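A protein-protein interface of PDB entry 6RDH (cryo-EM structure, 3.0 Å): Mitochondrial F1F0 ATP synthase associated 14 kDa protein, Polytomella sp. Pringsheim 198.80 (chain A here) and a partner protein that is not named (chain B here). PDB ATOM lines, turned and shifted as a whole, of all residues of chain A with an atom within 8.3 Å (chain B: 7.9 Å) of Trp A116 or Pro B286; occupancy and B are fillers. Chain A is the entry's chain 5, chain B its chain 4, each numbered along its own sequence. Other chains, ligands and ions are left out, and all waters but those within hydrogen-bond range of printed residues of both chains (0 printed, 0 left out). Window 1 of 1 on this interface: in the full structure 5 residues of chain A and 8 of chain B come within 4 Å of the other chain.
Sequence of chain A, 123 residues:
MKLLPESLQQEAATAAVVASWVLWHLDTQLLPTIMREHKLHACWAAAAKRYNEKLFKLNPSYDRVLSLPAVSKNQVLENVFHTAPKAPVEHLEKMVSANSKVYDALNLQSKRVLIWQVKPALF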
ATOM      1  N   ALA A 105      22.607   9.729 -12.300  1.00  0.00           N
ATOM      2  CA  ALA A 105      22.535  11.000 -11.610  1.00  0.00           C
ATOM      3  C   ALA A 105      23.883  11.528 -11.162  1.00  0.00           C
ATOM      4  O   ALA A 105      24.047  12.743 -11.070  1.00  0.00           O
ATOM      5  CB  ALA A 105      21.615  10.893 -10.404  1.00  0.00           C
ATOM      6  N   ASN A 107      27.554  10.823 -11.905  1.00  0.00           N
ATOM      7  CA  ASN A 107      28.789  10.285 -12.467  1.00  0.00           C
ATOM      8  C   ASN A 107      29.835  11.302 -12.922  1.00  0.00           C
ATOM      9  O   ASN A 107      31.025  10.973 -12.862  1.00  0.00           O
ATOM     10  CB  ASN A 107      28.503   9.377 -13.663  1.00  0.00           C
ATOM     11  CG  ASN A 107      29.659   8.474 -13.955  1.00  0.00           C
ATOM     12  OD1 ASN A 107      30.249   7.916 -13.040  1.00  0.00           O
ATOM     13  ND2 ASN A 107      30.072   8.419 -15.209  1.00  0.00           N
ATOM     14  N   LEU A 108      29.425  12.493 -13.382  1.00  0.00           N
ATOM     15  CA  LEU A 108      30.146  13.544 -14.122  1.00  0.00           C
ATOM     16  C   LEU A 108      30.395  13.186 -15.579  1.00  0.00           C
ATOM     17  O   LEU A 108      30.810  14.047 -16.356  1.00  0.00           O
ATOM     18  CB  LEU A 108      31.516  13.943 -13.550  1.00  0.00           C
ATOM     19  CG  LEU A 108      31.806  14.583 -12.203  1.00  0.00           C
ATOM     20  CD1 LEU A 108      32.389  13.535 -11.316  1.00  0.00           C
ATOM     21  CD2 LEU A 108      32.770  15.740 -12.361  1.00  0.00           C
ATOM     22  N   GLN A 109      30.146  11.949 -15.975  1.00  0.00           N
ATOM     23  CA  GLN A 109      30.216  11.581 -17.377  1.00  0.00           C
ATOM     24  C   GLN A 109      28.897  11.032 -17.870  1.00  0.00           C
ATOM     25  O   GLN A 109      28.775  10.722 -19.057  1.00  0.00           O
ATOM     26  CB  GLN A 109      31.329  10.558 -17.622  1.00  0.00           C
ATOM     27  CG  GLN A 109      32.685  11.185 -17.884  1.00  0.00           C
ATOM     28  CD  GLN A 109      33.534  11.301 -16.634  1.00  0.00           C
ATOM     29  OE1 GLN A 109      33.730  10.328 -15.908  1.00  0.00           O
ATOM     30  NE2 GLN A 109      34.043  12.499 -16.376  1.00  0.00           N
ATOM     31  N   SER A 110      27.920  10.898 -16.985  1.00  0.00           N
ATOM     32  CA  SER A 110      26.577  10.539 -17.387  1.00  0.00           C
ATOM     33  C   SER A 110      25.963  11.650 -18.207  1.00  0.00           C
ATOM     34  O   SER A 110      26.245  12.827 -17.999  1.00  0.00           O
ATOM     35  CB  SER A 110      25.702  10.287 -16.180  1.00  0.00           C
ATOM     36  OG  SER A 110      24.360  10.302 -16.598  1.00  0.00           O
ATOM     37  N   LYS A 111      25.102  11.263 -19.138  1.00  0.00           N
ATOM     38  CA  LYS A 111      24.500  12.236 -20.035  1.00  0.00           C
ATOM     39  C   LYS A 111      23.531  13.143 -19.291  1.00  0.00           C
ATOM     40  O   LYS A 111      23.592  14.366 -19.427  1.00  0.00           O
ATOM     41  CB  LYS A 111      23.813  11.505 -21.182  1.00  0.00           C
ATOM     42  CG  LYS A 111      23.178  12.395 -22.198  1.00  0.00           C
ATOM     43  CD  LYS A 111      22.685  11.600 -23.386  1.00  0.00           C
ATOM     44  CE  LYS A 111      23.837  11.212 -24.292  1.00  0.00           C
ATOM     45  NZ  LYS A 111      24.412  12.394 -24.982  1.00  0.00           N
ATOM     46  N   ARG A 112      22.633  12.569 -18.498  1.00  0.00           N
ATOM     47  CA  ARG A 112      21.737  13.368 -17.663  1.00  0.00           C
ATOM     48  C   ARG A 112      22.207  13.405 -16.211  1.00  0.00           C
ATOM     49  O   ARG A 112      21.506  12.993 -15.301  1.00  0.00           O
ATOM     50  CB  ARG A 112      20.312  12.846 -17.771  1.00  0.00           C
ATOM     51  CG  ARG A 112      20.173  11.349 -17.908  1.00  0.00           C
ATOM     52  CD  ARG A 112      18.704  10.976 -17.812  1.00  0.00           C
ATOM     53  NE  ARG A 112      18.509   9.618 -17.325  1.00  0.00           N
ATOM     54  CZ  ARG A 112      17.450   9.227 -16.624  1.00  0.00           C
ATOM     55  NH1 ARG A 112      17.344   7.972 -16.216  1.00  0.00           N
ATOM     56  NH2 ARG A 112      16.504  10.097 -16.309  1.00  0.00           N
ATOM     57  N   VAL A 113      23.389  13.968 -16.001  1.00  0.00           N
ATOM     58  CA  VAL A 113      23.981  14.068 -14.672  1.00  0.00           C
ATOM     59  C   VAL A 113      23.321  15.210 -13.908  1.00  0.00           C
ATOM     60  O   VAL A 113      22.836  16.180 -14.497  1.00  0.00           O
ATOM     61  CB  VAL A 113      25.513  14.236 -14.803  1.00  0.00           C
ATOM     62  CG1 VAL A 113      25.869  15.539 -15.444  1.00  0.00           C
ATOM     63  CG2 VAL A 113      26.228  14.070 -13.482  1.00  0.00           C
ATOM     64  N   LEU A 114      23.249  15.075 -12.582  1.00  0.00           N
ATOM     65  CA  LEU A 114      22.640  16.072 -11.711  1.00  0.00           C
ATOM     66  C   LEU A 114      23.646  16.976 -11.022  1.00  0.00           C
ATOM     67  O   LEU A 114      23.353  17.483  -9.940  1.00  0.00           O
ATOM     68  CB  LEU A 114      21.781  15.408 -10.641  1.00  0.00           C
ATOM     69  CG  LEU A 114      20.298  15.166 -10.873  1.00  0.00           C
ATOM     70  CD1 LEU A 114      20.029  14.073 -11.878  1.00  0.00           C
ATOM     71  CD2 LEU A 114      19.671  14.840  -9.543  1.00  0.00           C
ATOM     72  N   ILE A 115      24.825  17.190 -11.595  1.00  0.00           N
ATOM     73  CA  ILE A 115      25.748  18.092 -10.919  1.00  0.00           C
ATOM     74  C   ILE A 115      25.448  19.537 -11.298  1.00  0.00           C
ATOM     75  O   ILE A 115      25.618  20.446 -10.482  1.00  0.00           O
ATOM     76  CB  ILE A 115      27.202  17.678 -11.210  1.00  0.00           C
ATOM     77  CG1 ILE A 115      28.208  18.597 -10.523  1.00  0.00           C
ATOM     78  CG2 ILE A 115      27.474  17.622 -12.689  1.00  0.00           C
ATOM     79  CD1 ILE A 115      28.080  18.631  -9.031  1.00  0.00           C
ATOM     80  N   TRP A 116      24.934  19.782 -12.496  1.00  0.00           N
ATOM     81  CA  TRP A 116      24.635  21.143 -12.906  1.00  0.00           C
ATOM     82  C   TRP A 116      23.255  21.600 -12.476  1.00  0.00           C
ATOM     83  O   TRP A 116      22.915  22.764 -12.688  1.00  0.00           O
ATOM     84  CB  TRP A 116      24.796  21.271 -14.417  1.00  0.00           C
ATOM     85  CG  TRP A 116      26.065  20.652 -14.868  1.00  0.00           C
ATOM     86  CD1 TRP A 116      26.209  19.494 -15.554  1.00  0.00           C
ATOM     87  CD2 TRP A 116      27.382  21.140 -14.621  1.00  0.00           C
ATOM     88  NE1 TRP A 116      27.532  19.233 -15.766  1.00  0.00           N
ATOM     89  CE2 TRP A 116      28.274  20.231 -15.196  1.00  0.00           C
ATOM     90  CE3 TRP A 116      27.892  22.264 -13.973  1.00  0.00           C
ATOM     91  CZ2 TRP A 116      29.645  20.410 -15.151  1.00  0.00           C
ATOM     92  CZ3 TRP A 116      29.248  22.437 -13.921  1.00  0.00           C
ATOM     93  CH2 TRP A 116      30.113  21.519 -14.510  1.00  0.00           C
ATOM     94  N   GLN A 117      22.459  20.725 -11.877  1.00  0.00           N
ATOM     95  CA  GLN A 117      21.195  21.115 -11.288  1.00  0.00           C
ATOM     96  C   GLN A 117      21.319  21.373  -9.805  1.00  0.00           C
ATOM     97  O   GLN A 117      20.405  21.934  -9.206  1.00  0.00           O
ATOM     98  CB  GLN A 117      20.149  20.028 -11.493  1.00  0.00           C
ATOM     99  CG  GLN A 117      20.135  19.435 -12.853  1.00  0.00           C
ATOM    100  CD  GLN A 117      19.025  18.445 -13.006  1.00  0.00           C
ATOM    101  OE1 GLN A 117      18.205  18.284 -12.112  1.00  0.00           O
ATOM    102  NE2 GLN A 117      18.999  17.750 -14.131  1.00  0.00           N
ATOM    103  N   VAL A 118      22.427  20.969  -9.215  1.00  0.00           N
ATOM    104  CA  VAL A 118      22.600  20.935  -7.776  1.00  0.00           C
ATOM    105  C   VAL A 118      23.628  21.966  -7.325  1.00  0.00           C
ATOM    106  O   VAL A 118      23.340  22.814  -6.482  1.00  0.00           O
ATOM    107  CB  VAL A 118      22.970  19.507  -7.319  1.00  0.00           C
ATOM    108  CG1 VAL A 118      23.589  19.494  -5.980  1.00  0.00           C
ATOM    109  CG2 VAL A 118      21.726  18.673  -7.276  1.00  0.00           C
ATOM    110  N   LYS A 119      24.826  21.925  -7.893  1.00  0.00           N
ATOM    111  CA  LYS A 119      25.814  22.986  -7.751  1.00  0.00           C
ATOM    112  C   LYS A 119      25.885  23.623  -9.123  1.00  0.00           C
ATOM    113  O   LYS A 119      26.637  23.143  -9.981  1.00  0.00           O
ATOM    114  CB  LYS A 119      27.174  22.438  -7.325  1.00  0.00           C
ATOM    115  CG  LYS A 119      27.257  22.078  -5.864  1.00  0.00           C
ATOM    116  CD  LYS A 119      27.018  23.304  -5.018  1.00  0.00           C
ATOM    117  CE  LYS A 119      27.294  23.040  -3.557  1.00  0.00           C
ATOM    118  NZ  LYS A 119      28.722  22.698  -3.324  1.00  0.00           N
ATOM    119  N   PRO A 120      25.113  24.708  -9.380  1.00  0.00           N
ATOM    120  CA  PRO A 120      24.672  25.022 -10.748  1.00  0.00           C
ATOM    121  C   PRO A 120      25.754  25.309 -11.776  1.00  0.00           C
ATOM    122  O   PRO A 120      25.900  24.510 -12.705  1.00  0.00           O
ATOM    123  CB  PRO A 120      23.778  26.250 -10.540  1.00  0.00           C
ATOM    124  CG  PRO A 120      24.096  26.759  -9.218  1.00  0.00           C
ATOM    125  CD  PRO A 120      24.501  25.607  -8.396  1.00  0.00           C
ATOM    126  N   ALA A 121      26.503  26.402 -11.601  1.00  0.00           N
ATOM    127  CA  ALA A 121      27.765  26.726 -12.266  1.00  0.00           C
ATOM    128  C   ALA A 121      28.218  28.061 -11.719  1.00  0.00           C
ATOM    129  O   ALA A 121      27.541  28.645 -10.873  1.00  0.00           O
ATOM    130  CB  ALA A 121      27.673  26.835 -13.787  1.00  0.00           C
ATOM    131  N   LEU A 122      29.350  28.557 -12.197  1.00  0.00           N
ATOM    132  CA  LEU A 122      29.677  29.974 -12.076  1.00  0.00           C
ATOM    133  C   LEU A 122      30.358  30.377 -13.381  1.00  0.00           C
ATOM    134  O   LEU A 122      31.554  30.191 -13.580  1.00  0.00           O
ATOM    135  CB  LEU A 122      30.559  30.283 -10.873  1.00  0.00           C
ATOM    136  CG  LEU A 122      29.864  30.697  -9.596  1.00  0.00           C
ATOM    137  CD1 LEU A 122      30.862  30.766  -8.486  1.00  0.00           C
ATOM    138  CD2 LEU A 122      29.302  32.042  -9.853  1.00  0.00           C
ATOM    139  N   PHE B 278      18.513  23.431 -21.328  1.00  0.00           N
ATOM    140  CA  PHE B 278      19.557  23.168 -20.342  1.00  0.00           C
ATOM    141  C   PHE B 278      19.871  21.688 -20.273  1.00  0.00           C
ATOM    142  O   PHE B 278      21.042  21.296 -20.222  1.00  0.00           O
ATOM    143  CB  PHE B 278      19.121  23.676 -18.970  1.00  0.00           C
ATOM    144  CG  PHE B 278      20.236  23.788 -17.975  1.00  0.00           C
ATOM    145  CD1 PHE B 278      20.573  22.729 -17.156  1.00  0.00           C
ATOM    146  CD2 PHE B 278      20.930  24.966 -17.840  1.00  0.00           C
ATOM    147  CE1 PHE B 278      21.583  22.838 -16.244  1.00  0.00           C
ATOM    148  CE2 PHE B 278      21.945  25.078 -16.924  1.00  0.00           C
ATOM    149  CZ  PHE B 278      22.270  24.012 -16.130  1.00  0.00           C
ATOM    150  N   ALA B 280      19.375  19.553 -22.742  1.00  0.00           N
ATOM    151  CA  ALA B 280      20.011  19.178 -24.001  1.00  0.00           C
ATOM    152  C   ALA B 280      21.481  19.585 -24.047  1.00  0.00           C
ATOM    153  O   ALA B 280      22.335  18.800 -24.475  1.00  0.00           O
ATOM    154  CB  ALA B 280      19.249  19.796 -25.169  1.00  0.00           C
ATOM    155  N   SER B 281      21.806  20.797 -23.598  1.00  0.00           N
ATOM    156  CA  SER B 281      23.188  21.250 -23.660  1.00  0.00           C
ATOM    157  C   SER B 281      24.055  20.638 -22.571  1.00  0.00           C
ATOM    158  O   SER B 281      25.278  20.623 -22.716  1.00  0.00           O
ATOM    159  CB  SER B 281      23.264  22.767 -23.572  1.00  0.00           C
ATOM    160  OG  SER B 281      22.912  23.208 -22.279  1.00  0.00           O
ATOM    161  N   VAL B 282      23.466  20.147 -21.481  1.00  0.00           N
ATOM    162  CA  VAL B 282      24.254  19.318 -20.579  1.00  0.00           C
ATOM    163  C   VAL B 282      24.428  17.933 -21.183  1.00  0.00           C
ATOM    164  O   VAL B 282      25.493  17.323 -21.050  1.00  0.00           O
ATOM    165  CB  VAL B 282      23.604  19.288 -19.184  1.00  0.00           C
ATOM    166  CG1 VAL B 282      24.205  18.222 -18.285  1.00  0.00           C
ATOM    167  CG2 VAL B 282      23.768  20.632 -18.527  1.00  0.00           C
ATOM    168  N   ALA B 283      23.424  17.451 -21.921  1.00  0.00           N
ATOM    169  CA  ALA B 283      23.512  16.145 -22.557  1.00  0.00           C
ATOM    170  C   ALA B 283      24.585  16.098 -23.633  1.00  0.00           C
ATOM    171  O   ALA B 283      25.205  15.052 -23.836  1.00  0.00           O
ATOM    172  CB  ALA B 283      22.160  15.771 -23.155  1.00  0.00           C
ATOM    173  N   GLU B 284      24.835  17.210 -24.319  1.00  0.00           N
ATOM    174  CA  GLU B 284      25.854  17.183 -25.359  1.00  0.00           C
ATOM    175  C   GLU B 284      27.265  17.413 -24.822  1.00  0.00           C
ATOM    176  O   GLU B 284      28.227  17.157 -25.548  1.00  0.00           O
ATOM    177  CB  GLU B 284      25.525  18.202 -26.452  1.00  0.00           C
ATOM    178  CG  GLU B 284      25.640  19.658 -26.049  1.00  0.00           C
ATOM    179  CD  GLU B 284      26.961  20.276 -26.460  1.00  0.00           C
ATOM    180  OE1 GLU B 284      27.631  19.696 -27.337  1.00  0.00           O
ATOM    181  OE2 GLU B 284      27.331  21.333 -25.910  1.00  0.00           O
ATOM    182  N   ALA B 285      27.417  17.884 -23.587  1.00  0.00           N
ATOM    183  CA  ALA B 285      28.739  18.104 -22.994  1.00  0.00           C
ATOM    184  C   ALA B 285      28.640  18.033 -21.479  1.00  0.00           C
ATOM    185  O   ALA B 285      28.601  19.057 -20.793  1.00  0.00           O
ATOM    186  CB  ALA B 285      29.320  19.448 -23.426  1.00  0.00           C
ATOM    187  N   PRO B 286      28.620  16.824 -20.913  1.00  0.00           N
ATOM    188  CA  PRO B 286      28.291  16.698 -19.489  1.00  0.00           C
ATOM    189  C   PRO B 286      29.429  16.964 -18.534  1.00  0.00           C
ATOM    190  O   PRO B 286      29.161  17.264 -17.367  1.00  0.00           O
ATOM    191  CB  PRO B 286      27.821  15.252 -19.377  1.00  0.00           C
ATOM    192  CG  PRO B 286      28.542  14.552 -20.434  1.00  0.00           C
ATOM    193  CD  PRO B 286      28.707  15.508 -21.566  1.00  0.00           C
ATOM    194  N   ALA B 287      30.676  16.848 -18.958  1.00  0.00           N
ATOM    195  CA  ALA B 287      31.775  17.108 -18.045  1.00  0.00           C
ATOM    196  C   ALA B 287      32.212  18.560 -18.049  1.00  0.00           C
ATOM    197  O   ALA B 287      33.080  18.928 -17.254  1.00  0.00           O
ATOM    198  CB  ALA B 287      32.969  16.217 -18.380  1.00  0.00           C
ATOM    199  N   SER B 288      31.639  19.390 -18.920  1.00  0.00           N
ATOM    200  CA  SER B 288      31.971  20.804 -18.964  1.00  0.00           C
ATOM    201  C   SER B 288      30.841  21.710 -18.510  1.00  0.00           C
ATOM    202  O   SER B 288      31.109  22.847 -18.118  1.00  0.00           O
ATOM    203  CB  SER B 288      32.387  21.216 -20.382  1.00  0.00           C
ATOM    204  OG  SER B 288      31.273  21.243 -21.253  1.00  0.00           O
ATOM    205  N   GLY B 289      29.598  21.246 -18.550  1.00  0.00           N
ATOM    206  CA  GLY B 289      28.476  22.054 -18.149  1.00  0.00           C
ATOM    207  C   GLY B 289      27.601  22.444 -19.318  1.00  0.00           C
ATOM    208  O   GLY B 289      27.732  21.911 -20.421  1.00  0.00           O
ATOM    209  N   PRO B 290      26.679  23.375 -19.095  1.00  0.00           N
ATOM    210  CA  PRO B 290      25.878  23.884 -20.206  1.00  0.00           C
ATOM    211  C   PRO B 290      26.709  24.801 -21.080  1.00  0.00           C
ATOM    212  O   PRO B 290      27.654  25.447 -20.623  1.00  0.00           O
ATOM    213  CB  PRO B 290      24.754  24.646 -19.506  1.00  0.00           C
ATOM    214  CG  PRO B 290      25.349  25.080 -18.249  1.00  0.00           C
ATOM    215  CD  PRO B 290      26.295  24.002 -17.824  1.00  0.00           C
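The side-chain amino group (NZ) of Lys A111 lies within hydrogen-bond range of the backbone carbonyl oxygen (O) of Ala B283, 3.0 Å away.
NE1 of Trp A116 sits at hydrogen-bond distance from O of Pro B286.
The backbone carbonyl oxygen (O) of Phe B278 sits at hydrogen-bond distance from the side-chain hydroxyl (OG) of Ser B281, at 3.4 Å.
O of Ala B285 lies close to OG of Ser B288, 3.5 Å away.
N of Arg A112 sits at hydrogen-bond distance from OG of Ser A110, 3.4 Å away.
Among the printed residues, pairs that only touch across the chains: Ser A110 with Pro B286 (3.2 Å), Trp A116 with Gly B289 (3.5 Å), Trp A116 with Val B282 (3.6 Å), Leu A108 with Ala B287 (3.6 Å), Trp A116 with Phe B278 (3.7 Å), Leu A108 with Pro B286 (3.8 Å), Trp A116 with Ser B288 (3.8 Å) and Lys A111 with Val B282 (3.9 Å).
Printed residues of chain B within 4 Å of Ser A110: Pro B286.
Of the printed residues of chain B, Lys A111 touches Val B282 and Ala B283.
Trp A116 touches just these residues of chain B: Phe B278, Val B282, Pro B286, Ser B288 and Gly B289.
Of the printed residues of chain A, Ala B283 touches Lys A111 (3.0 Å).
Of chain A, only Leu A108 (3.8 Å), Ser A110 (3.2 Å) and Trp A116 (3.0 Å) come within 4 Å of Pro B286.
Of the printed residues of chain A, Gly B289 touches Trp A116.
The nearest residue of chain B that does not touch Trp A116 is Ala B287 (4.3 Å).
The nearest residue of chain A that does not touch Pro B286 is Gln A109 (4.1 Å).
Of the 17 printed residues of chain A, 4 touch a printed residue of chain B.
Hydrophobic or aromatic side chains of chain A that line the printed part of chain B: Trp A116.
Along chain A the printed residues that touch a printed residue of chain B span positions 108 to 116.
Hydrophobic or aromatic side chains of chain B that line the printed part of chain A: Phe B278, Val B282, Ala B283, Pro B286 and Ala B287.
Among the printed residues, no Asp or Glu carboxylate lies within 4 Å of a Lys or Arg side-chain nitrogen of the other chain.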
